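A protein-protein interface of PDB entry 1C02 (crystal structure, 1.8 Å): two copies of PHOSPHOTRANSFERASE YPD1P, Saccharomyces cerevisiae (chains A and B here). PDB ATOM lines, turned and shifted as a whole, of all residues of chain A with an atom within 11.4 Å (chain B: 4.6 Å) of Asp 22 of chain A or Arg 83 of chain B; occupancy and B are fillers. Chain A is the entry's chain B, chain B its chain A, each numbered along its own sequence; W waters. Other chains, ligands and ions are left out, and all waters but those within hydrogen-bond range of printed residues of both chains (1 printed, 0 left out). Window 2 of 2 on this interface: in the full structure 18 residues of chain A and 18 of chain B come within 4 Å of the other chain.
Among the printed residues, pairs that only touch across the chains: Met 19 of chain A with Glu 82 of chain B (3.8 Å) and Asp 23 of chain A with Gln 85 of chain B (3.7 Å).
Of chain B, only Glu 82, Arg 83 and Asn 86 come within 4 Å of Asp 22 of chain A.
Arg 83 of chain B touches one residue of chain A.
No residue of chain A comes within 4 Å of Trp 79 of chain B.
No residue of chain A comes within 4 Å of Val 80 of chain B.
Glu 82 of chain B touches just these residues of chain A: Met 19 and Asp 22.
No residue of chain A comes within 4 Å of Ile 84 of chain B.
Gln 85 of chain B touches just one residue of chain A: Asp 23 (3.7 Å).
Of chain A, only Asp 22 (3.3 Å) comes within 4 Å of Asn 86 of chain B.
No residue of chain A comes within 4 Å of Leu 87 of chain B.
No residue of chain A comes within 4 Å of Gln 92 of chain B.
Of the printed residues of chain B, Asp 23 of chain A touches Gln 85 (3.7 Å).
Printed residues of chain B within 4 Å of Met 19 of chain A: Glu 82.
The nearest residue of chain A that does not touch Arg 83 of chain B is Met 19 of chain A (6.9 Å).
The nearest printed residue of chain B that does not touch Asp 23 of chain A is Glu 82 of chain B (5.2 Å).
NH1 of Arg 83 of chain B is in salt-bridge range of OD1 of Asp 22 of chain A (3.5 Å).
OD1 of Asn 86 of chain B lies close to O of Asp 22 of chain A, at 3.3 Å.
The side-chain carboxylate of Glu 82 of chain B lies close to the side-chain carboxylate of Asp 22 of chain A (3.2 Å).
The side-chain carboxylate of Glu 82 of chain B is in salt-bridge range of the guanidinium group of Arg 83 of chain B (2.8 Å).
The side-chain amide nitrogen (ND2) of Asn 86 of chain B is in hydrogen-bond range of the backbone carbonyl oxygen (O) of Glu 82 of chain B, 3.5 Å away.
NH1 of Arg 83 of chain B sits close to ND2 of Asn 86 of chain B (3.2 Å).
The side-chain amide oxygen of Gln 92 of chain B lies within hydrogen-bond range of the guanidinium group of Arg 83 of chain B, 2.9 Å away.
The backbone carbonyl oxygen of Asn 86 of chain B lies within hydrogen-bond range of the backbone NH of Met 91 of chain B.
The side-chain amide nitrogen (ND2) of Asn 86 of chain B is in hydrogen-bond range of the side-chain amide oxygen (OE1) of Gln 92 of chain B (3.1 Å).
No position is printed for both chains.
Of the 5 pairs that touch across the chains among the printed residues, none has its exchanged pair printed and touching as well.
Water W1 bridges the side-chain carboxylate (OE1) of Glu 82 of chain B (2.5 Å) and the backbone carbonyl oxygen (O) of Met 19 of chain A (2.6 Å).
Printed residues of chain A that touch a printed residue of chain B: Met 19, Asp 22 and Asp 23.
Hydrophobic or aromatic side chains of chain A within 4 Å of the printed part of chain B: Met 19.
Along chain A the printed residues that touch a printed residue of chain B span positions 19 to 23.
Printed residues of chain B that touch a printed residue of chain A: Glu 82, Arg 83, Gln 85 and Asn 86.
Among the printed residues, Asp or Glu carboxylates within 4 Å of a Lys or Arg side-chain nitrogen of the other chain: Asp 22 of chain A with Arg 83 of chain B (3.5 Å).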
ATOM      1  N   ASN A  14      28.650  27.793 -35.742  1.00  0.00           N
ATOM      2  CA  ASN A  14      27.520  26.875 -35.865  1.00  0.00           C
ATOM      3  C   ASN A  14      27.661  25.680 -34.931  1.00  0.00           C
ATOM      4  O   ASN A  14      26.660  25.148 -34.442  1.00  0.00           O
ATOM      5  CB  ASN A  14      27.378  26.373 -37.302  1.00  0.00           C
ATOM      6  CG  ASN A  14      26.543  27.301 -38.167  1.00  0.00           C
ATOM      7  OD1 ASN A  14      26.642  27.260 -39.393  1.00  0.00           O
ATOM      8  ND2 ASN A  14      25.727  28.154 -37.535  1.00  0.00           N
ATOM      9  N   GLU A  15      28.904  25.271 -34.673  1.00  0.00           N
ATOM     10  CA  GLU A  15      29.154  24.169 -33.754  1.00  0.00           C
ATOM     11  C   GLU A  15      28.743  24.545 -32.343  1.00  0.00           C
ATOM     12  O   GLU A  15      28.097  23.767 -31.648  1.00  0.00           O
ATOM     13  CB  GLU A  15      30.624  23.767 -33.795  1.00  0.00           C
ATOM     14  CG  GLU A  15      31.054  23.159 -35.126  1.00  0.00           C
ATOM     15  CD  GLU A  15      30.347  21.847 -35.448  1.00  0.00           C
ATOM     16  OE1 GLU A  15      30.317  21.473 -36.641  1.00  0.00           O
ATOM     17  OE2 GLU A  15      29.847  21.179 -34.514  1.00  0.00           O
ATOM     18  N   ILE A  16      29.003  25.792 -31.975  1.00  0.00           N
ATOM     19  CA  ILE A  16      28.621  26.309 -30.671  1.00  0.00           C
ATOM     20  C   ILE A  16      27.092  26.435 -30.607  1.00  0.00           C
ATOM     21  O   ILE A  16      26.479  26.094 -29.593  1.00  0.00           O
ATOM     22  CB  ILE A  16      29.298  27.697 -30.423  1.00  0.00           C
ATOM     23  CG1 ILE A  16      30.823  27.538 -30.413  1.00  0.00           C
ATOM     24  CG2 ILE A  16      28.771  28.349 -29.144  1.00  0.00           C
ATOM     25  CD1 ILE A  16      31.422  27.266 -29.049  1.00  0.00           C
ATOM     26  N   ILE A  17      26.475  26.852 -31.716  1.00  0.00           N
ATOM     27  CA  ILE A  17      25.028  27.085 -31.748  1.00  0.00           C
ATOM     28  C   ILE A  17      24.260  25.758 -31.791  1.00  0.00           C
ATOM     29  O   ILE A  17      23.132  25.671 -31.298  1.00  0.00           O
ATOM     30  CB  ILE A  17      24.633  27.976 -32.957  1.00  0.00           C
ATOM     31  CG1 ILE A  17      25.173  29.396 -32.747  1.00  0.00           C
ATOM     32  CG2 ILE A  17      23.110  28.044 -33.102  1.00  0.00           C
ATOM     33  CD1 ILE A  17      25.184  30.249 -33.998  1.00  0.00           C
ATOM     34  N   SER A  18      24.935  24.700 -32.237  1.00  0.00           N
ATOM     35  CA  SER A  18      24.384  23.346 -32.165  1.00  0.00           C
ATOM     36  C   SER A  18      23.952  22.979 -30.755  1.00  0.00           C
ATOM     37  O   SER A  18      23.034  22.187 -30.577  1.00  0.00           O
ATOM     38  CB  SER A  18      25.405  22.322 -32.652  1.00  0.00           C
ATOM     39  OG  SER A  18      25.326  22.182 -34.056  1.00  0.00           O
ATOM     40  N   MET A  19      24.550  23.619 -29.755  1.00  0.00           N
ATOM     41  CA  MET A  19      24.305  23.255 -28.365  1.00  0.00           C
ATOM     42  C   MET A  19      23.207  24.065 -27.678  1.00  0.00           C
ATOM     43  O   MET A  19      22.919  23.856 -26.496  1.00  0.00           O
ATOM     44  CB  MET A  19      25.615  23.343 -27.581  1.00  0.00           C
ATOM     45  CG  MET A  19      26.725  22.490 -28.190  1.00  0.00           C
ATOM     46  SD  MET A  19      28.063  22.155 -27.046  1.00  0.00           S
ATOM     47  CE  MET A  19      27.347  20.803 -26.106  1.00  0.00           C
ATOM     48  N   ASP A  20      22.493  24.877 -28.454  1.00  0.00           N
ATOM     49  CA  ASP A  20      21.341  25.608 -27.937  1.00  0.00           C
ATOM     50  C   ASP A  20      20.102  24.724 -27.858  1.00  0.00           C
ATOM     51  O   ASP A  20      19.064  25.136 -27.345  1.00  0.00           O
ATOM     52  CB  ASP A  20      21.041  26.805 -28.831  1.00  0.00           C
ATOM     53  CG  ASP A  20      22.113  27.869 -28.752  1.00  0.00           C
ATOM     54  OD1 ASP A  20      22.292  28.615 -29.738  1.00  0.00           O
ATOM     55  OD2 ASP A  20      22.757  27.983 -27.689  1.00  0.00           O
ATOM     56  N   ASP A  21      20.216  23.514 -28.392  1.00  0.00           N
ATOM     57  CA  ASP A  21      19.080  22.616 -28.491  1.00  0.00           C
ATOM     58  C   ASP A  21      18.610  22.105 -27.134  1.00  0.00           C
ATOM     59  O   ASP A  21      17.408  22.028 -26.890  1.00  0.00           O
ATOM     60  CB  ASP A  21      19.419  21.452 -29.422  1.00  0.00           C
ATOM     61  CG  ASP A  21      19.509  21.881 -30.877  1.00  0.00           C
ATOM     62  OD1 ASP A  21      20.217  21.205 -31.660  1.00  0.00           O
ATOM     63  OD2 ASP A  21      18.885  22.911 -31.235  1.00  0.00           O
ATOM     64  N   ASP A  22      19.550  21.845 -26.229  1.00  0.00           N
ATOM     65  CA  ASP A  22      19.213  21.396 -24.883  1.00  0.00           C
ATOM     66  C   ASP A  22      19.574  22.425 -23.820  1.00  0.00           C
ATOM     67  O   ASP A  22      19.618  22.110 -22.635  1.00  0.00           O
ATOM     68  CB  ASP A  22      19.911  20.072 -24.588  1.00  0.00           C
ATOM     69  CG  ASP A  22      19.496  18.978 -25.545  1.00  0.00           C
ATOM     70  OD1 ASP A  22      20.370  18.194 -25.967  1.00  0.00           O
ATOM     71  OD2 ASP A  22      18.295  18.913 -25.892  1.00  0.00           O
ATOM     72  N   ASP A  23      19.774  23.667 -24.256  1.00  0.00           N
ATOM     73  CA  ASP A  23      20.129  24.782 -23.375  1.00  0.00           C
ATOM     74  C   ASP A  23      19.966  26.059 -24.203  1.00  0.00           C
ATOM     75  O   ASP A  23      20.937  26.600 -24.738  1.00  0.00           O
ATOM     76  CB  ASP A  23      21.585  24.633 -22.888  1.00  0.00           C
ATOM     77  CG  ASP A  23      21.967  25.657 -21.829  1.00  0.00           C
ATOM     78  OD1 ASP A  23      23.166  25.746 -21.487  1.00  0.00           O
ATOM     79  OD2 ASP A  23      21.083  26.392 -21.348  1.00  0.00           O
ATOM     80  N   SER A  24      18.732  26.544 -24.292  1.00  0.00           N
ATOM     81  CA  SER A  24      18.330  27.464 -25.358  1.00  0.00           C
ATOM     82  C   SER A  24      19.088  28.797 -25.445  1.00  0.00           C
ATOM     83  O   SER A  24      19.133  29.421 -26.511  1.00  0.00           O
ATOM     84  CB  SER A  24      16.816  27.725 -25.292  1.00  0.00           C
ATOM     85  OG  SER A  24      16.426  28.245 -24.033  1.00  0.00           O
ATOM     86  N   ASP A  25      19.703  29.226 -24.352  1.00  0.00           N
ATOM     87  CA  ASP A  25      20.421  30.488 -24.385  1.00  0.00           C
ATOM     88  C   ASP A  25      21.929  30.340 -24.276  1.00  0.00           C
ATOM     89  O   ASP A  25      22.625  31.298 -23.940  1.00  0.00           O
ATOM     90  CB  ASP A  25      19.905  31.411 -23.286  1.00  0.00           C
ATOM     91  CG  ASP A  25      18.584  32.053 -23.646  1.00  0.00           C
ATOM     92  OD1 ASP A  25      17.791  32.318 -22.722  1.00  0.00           O
ATOM     93  OD2 ASP A  25      18.333  32.282 -24.851  1.00  0.00           O
ATOM     94  N   PHE A  26      22.442  29.167 -24.635  1.00  0.00           N
ATOM     95  CA  PHE A  26      23.859  28.866 -24.443  1.00  0.00           C
ATOM     96  C   PHE A  26      24.770  29.794 -25.247  1.00  0.00           C
ATOM     97  O   PHE A  26      25.561  30.549 -24.673  1.00  0.00           O
ATOM     98  CB  PHE A  26      24.147  27.406 -24.805  1.00  0.00           C
ATOM     99  CG  PHE A  26      25.605  27.037 -24.738  1.00  0.00           C
ATOM    100  CD1 PHE A  26      26.322  27.176 -23.546  1.00  0.00           C
ATOM    101  CD2 PHE A  26      26.251  26.519 -25.856  1.00  0.00           C
ATOM    102  CE1 PHE A  26      27.657  26.798 -23.466  1.00  0.00           C
ATOM    103  CE2 PHE A  26      27.587  26.138 -25.791  1.00  0.00           C
ATOM    104  CZ  PHE A  26      28.294  26.276 -24.588  1.00  0.00           C
ATOM    105  N   SER A  27      24.628  29.759 -26.567  1.00  0.00           N
ATOM    106  CA  SER A  27      25.510  30.485 -27.462  1.00  0.00           C
ATOM    107  C   SER A  27      25.351  31.989 -27.298  1.00  0.00           C
ATOM    108  O   SER A  27      26.345  32.722 -27.263  1.00  0.00           O
ATOM    109  CB  SER A  27      25.244  30.076 -28.913  1.00  0.00           C
ATOM    110  OG  SER A  27      24.035  30.642 -29.386  1.00  0.00           O
ATOM    111  N   TRP B  79      29.295  17.275 -24.121  1.00  0.00           N
ATOM    112  CA  TRP B  79      28.015  16.579 -24.090  1.00  0.00           C
ATOM    113  C   TRP B  79      27.681  16.097 -22.678  1.00  0.00           C
ATOM    114  O   TRP B  79      26.585  16.353 -22.185  1.00  0.00           O
ATOM    115  CB  TRP B  79      28.023  15.401 -25.071  1.00  0.00           C
ATOM    116  CG  TRP B  79      26.714  14.664 -25.149  1.00  0.00           C
ATOM    117  CD1 TRP B  79      25.668  14.949 -25.961  1.00  0.00           C
ATOM    118  CD2 TRP B  79      26.326  13.526 -24.372  1.00  0.00           C
ATOM    119  NE1 TRP B  79      24.642  14.065 -25.737  1.00  0.00           N
ATOM    120  CE2 TRP B  79      25.018  13.188 -24.758  1.00  0.00           C
ATOM    121  CE3 TRP B  79      26.959  12.762 -23.382  1.00  0.00           C
ATOM    122  CZ2 TRP B  79      24.318  12.123 -24.185  1.00  0.00           C
ATOM    123  CZ3 TRP B  79      26.266  11.695 -22.811  1.00  0.00           C
ATOM    124  CH2 TRP B  79      24.957  11.390 -23.215  1.00  0.00           C
ATOM    125  N   VAL B  80      28.648  15.494 -21.990  1.00  0.00           N
ATOM    126  CA  VAL B  80      28.395  15.017 -20.638  1.00  0.00           C
ATOM    127  C   VAL B  80      28.134  16.184 -19.676  1.00  0.00           C
ATOM    128  O   VAL B  80      27.227  16.113 -18.844  1.00  0.00           O
ATOM    129  CB  VAL B  80      29.554  14.115 -20.113  1.00  0.00           C
ATOM    130  CG1 VAL B  80      29.231  13.580 -18.735  1.00  0.00           C
ATOM    131  CG2 VAL B  80      29.777  12.950 -21.052  1.00  0.00           C
ATOM    132  N   CYS B  81      28.820  17.311 -19.869  1.00  0.00           N
ATOM    133  CA  CYS B  81      28.563  18.494 -19.052  1.00  0.00           C
ATOM    134  C   CYS B  81      27.151  19.033 -19.260  1.00  0.00           C
ATOM    135  O   CYS B  81      26.503  19.482 -18.315  1.00  0.00           O
ATOM    136  CB  CYS B  81      29.593  19.581 -19.355  1.00  0.00           C
ATOM    137  SG  CYS B  81      31.213  19.198 -18.714  1.00  0.00           S
ATOM    138  N   GLU B  82      26.652  18.903 -20.484  1.00  0.00           N
ATOM    139  CA  GLU B  82      25.293  19.301 -20.828  1.00  0.00           C
ATOM    140  C   GLU B  82      24.280  18.409 -20.097  1.00  0.00           C
ATOM    141  O   GLU B  82      23.250  18.894 -19.619  1.00  0.00           O
ATOM    142  CB  GLU B  82      25.105  19.197 -22.346  1.00  0.00           C
ATOM    143  CG  GLU B  82      23.689  19.466 -22.862  1.00  0.00           C
ATOM    144  CD  GLU B  82      23.590  19.371 -24.372  1.00  0.00           C
ATOM    145  OE1 GLU B  82      23.766  20.403 -25.044  1.00  0.00           O
ATOM    146  OE2 GLU B  82      23.399  18.253 -24.893  1.00  0.00           O
ATOM    147  N   ARG B  83      24.616  17.129 -19.927  1.00  0.00           N
ATOM    148  CA  ARG B  83      23.746  16.210 -19.194  1.00  0.00           C
ATOM    149  C   ARG B  83      23.722  16.581 -17.727  1.00  0.00           C
ATOM    150  O   ARG B  83      22.649  16.746 -17.162  1.00  0.00           O
ATOM    151  CB  ARG B  83      24.197  14.755 -19.365  1.00  0.00           C
ATOM    152  CG  ARG B  83      24.344  14.316 -20.814  1.00  0.00           C
ATOM    153  CD  ARG B  83      23.028  13.917 -21.477  1.00  0.00           C
ATOM    154  NE  ARG B  83      22.133  15.048 -21.703  1.00  0.00           N
ATOM    155  CZ  ARG B  83      22.234  15.911 -22.707  1.00  0.00           C
ATOM    156  NH1 ARG B  83      21.324  16.861 -22.859  1.00  0.00           N
ATOM    157  NH2 ARG B  83      23.263  15.858 -23.533  1.00  0.00           N
ATOM    158  N   ILE B  84      24.888  16.892 -17.165  1.00  0.00           N
ATOM    159  CA  ILE B  84      24.974  17.279 -15.758  1.00  0.00           C
ATOM    160  C   ILE B  84      24.142  18.511 -15.471  1.00  0.00           C
ATOM    161  O   ILE B  84      23.364  18.509 -14.525  1.00  0.00           O
ATOM    162  CB  ILE B  84      26.416  17.531 -15.315  1.00  0.00           C
ATOM    163  CG1 ILE B  84      27.179  16.206 -15.283  1.00  0.00           C
ATOM    164  CG2 ILE B  84      26.444  18.167 -13.929  1.00  0.00           C
ATOM    165  CD1 ILE B  84      28.664  16.360 -15.031  1.00  0.00           C
ATOM    166  N   GLN B  85      24.240  19.526 -16.325  1.00  0.00           N
ATOM    167  CA  GLN B  85      23.343  20.681 -16.253  1.00  0.00           C
ATOM    168  C   GLN B  85      21.848  20.329 -16.231  1.00  0.00           C
ATOM    169  O   GLN B  85      21.114  20.801 -15.373  1.00  0.00           O
ATOM    170  CB  GLN B  85      23.591  21.609 -17.431  1.00  0.00           C
ATOM    171  CG  GLN B  85      24.699  22.581 -17.236  1.00  0.00           C
ATOM    172  CD  GLN B  85      24.686  23.636 -18.315  1.00  0.00           C
ATOM    173  OE1 GLN B  85      24.166  24.726 -18.119  1.00  0.00           O
ATOM    174  NE2 GLN B  85      25.169  23.278 -19.490  1.00  0.00           N
ATOM    175  N   ASN B  86      21.378  19.598 -17.236  1.00  0.00           N
ATOM    176  CA  ASN B  86      19.958  19.282 -17.329  1.00  0.00           C
ATOM    177  C   ASN B  86      19.444  18.356 -16.213  1.00  0.00           C
ATOM    178  O   ASN B  86      18.252  18.360 -15.911  1.00  0.00           O
ATOM    179  CB  ASN B  86      19.638  18.685 -18.700  1.00  0.00           C
ATOM    180  CG  ASN B  86      19.809  19.686 -19.826  1.00  0.00           C
ATOM    181  OD1 ASN B  86      19.792  20.894 -19.609  1.00  0.00           O
ATOM    182  ND2 ASN B  86      20.062  19.184 -21.020  1.00  0.00           N
ATOM    183  N   LEU B  87      20.333  17.584 -15.588  1.00  0.00           N
ATOM    184  CA  LEU B  87      19.976  16.817 -14.391  1.00  0.00           C
ATOM    185  C   LEU B  87      19.893  17.726 -13.165  1.00  0.00           C
ATOM    186  O   LEU B  87      18.984  17.595 -12.349  1.00  0.00           O
ATOM    187  CB  LEU B  87      21.000  15.713 -14.144  1.00  0.00           C
ATOM    188  CG  LEU B  87      21.084  14.581 -15.168  1.00  0.00           C
ATOM    189  CD1 LEU B  87      22.418  13.851 -15.047  1.00  0.00           C
ATOM    190  CD2 LEU B  87      19.932  13.623 -14.953  1.00  0.00           C
ATOM    191  N   MET B  91      15.465  18.633 -15.622  1.00  0.00           N
ATOM    192  CA  MET B  91      14.861  18.506 -16.937  1.00  0.00           C
ATOM    193  C   MET B  91      15.084  17.128 -17.529  1.00  0.00           C
ATOM    194  O   MET B  91      14.423  16.755 -18.490  1.00  0.00           O
ATOM    195  CB  MET B  91      15.425  19.565 -17.871  1.00  0.00           C
ATOM    196  CG  MET B  91      15.198  20.977 -17.377  1.00  0.00           C
ATOM    197  SD  MET B  91      15.196  22.161 -18.721  1.00  0.00           S
ATOM    198  CE  MET B  91      16.908  22.054 -19.272  1.00  0.00           C
ATOM    199  N   GLN B  92      16.066  16.405 -16.993  1.00  0.00           N
ATOM    200  CA  GLN B  92      16.372  15.043 -17.422  1.00  0.00           C
ATOM    201  C   GLN B  92      16.405  14.111 -16.219  1.00  0.00           C
ATOM    202  O   GLN B  92      16.592  14.561 -15.095  1.00  0.00           O
ATOM    203  CB  GLN B  92      17.711  15.010 -18.159  1.00  0.00           C
ATOM    204  CG  GLN B  92      17.580  15.350 -19.643  1.00  0.00           C
ATOM    205  CD  GLN B  92      18.915  15.591 -20.330  1.00  0.00           C
ATOM    206  OE1 GLN B  92      18.988  16.321 -21.317  1.00  0.00           O
ATOM    207  NE2 GLN B  92      19.971  14.980 -19.815  1.00  0.00           N
ATOM    208  N   PHE B  95      20.568   8.760 -17.109  1.00  0.00           N
ATOM    209  CA  PHE B  95      21.907   8.847 -17.677  1.00  0.00           C
ATOM    210  C   PHE B  95      22.387   7.423 -17.965  1.00  0.00           C
ATOM    211  O   PHE B  95      22.239   6.533 -17.128  1.00  0.00           O
ATOM    212  CB  PHE B  95      22.861   9.540 -16.692  1.00  0.00           C
ATOM    213  CG  PHE B  95      24.215   9.859 -17.274  1.00  0.00           C
ATOM    214  CD1 PHE B  95      24.397  10.982 -18.067  1.00  0.00           C
ATOM    215  CD2 PHE B  95      25.287   9.003 -17.081  1.00  0.00           C
ATOM    216  CE1 PHE B  95      25.637  11.241 -18.674  1.00  0.00           C
ATOM    217  CE2 PHE B  95      26.519   9.252 -17.678  1.00  0.00           C
ATOM    218  CZ  PHE B  95      26.693  10.371 -18.479  1.00  0.00           C
HETATM  219  O   HOH W   1      23.992  22.794 -24.342  1.00  0.00           O
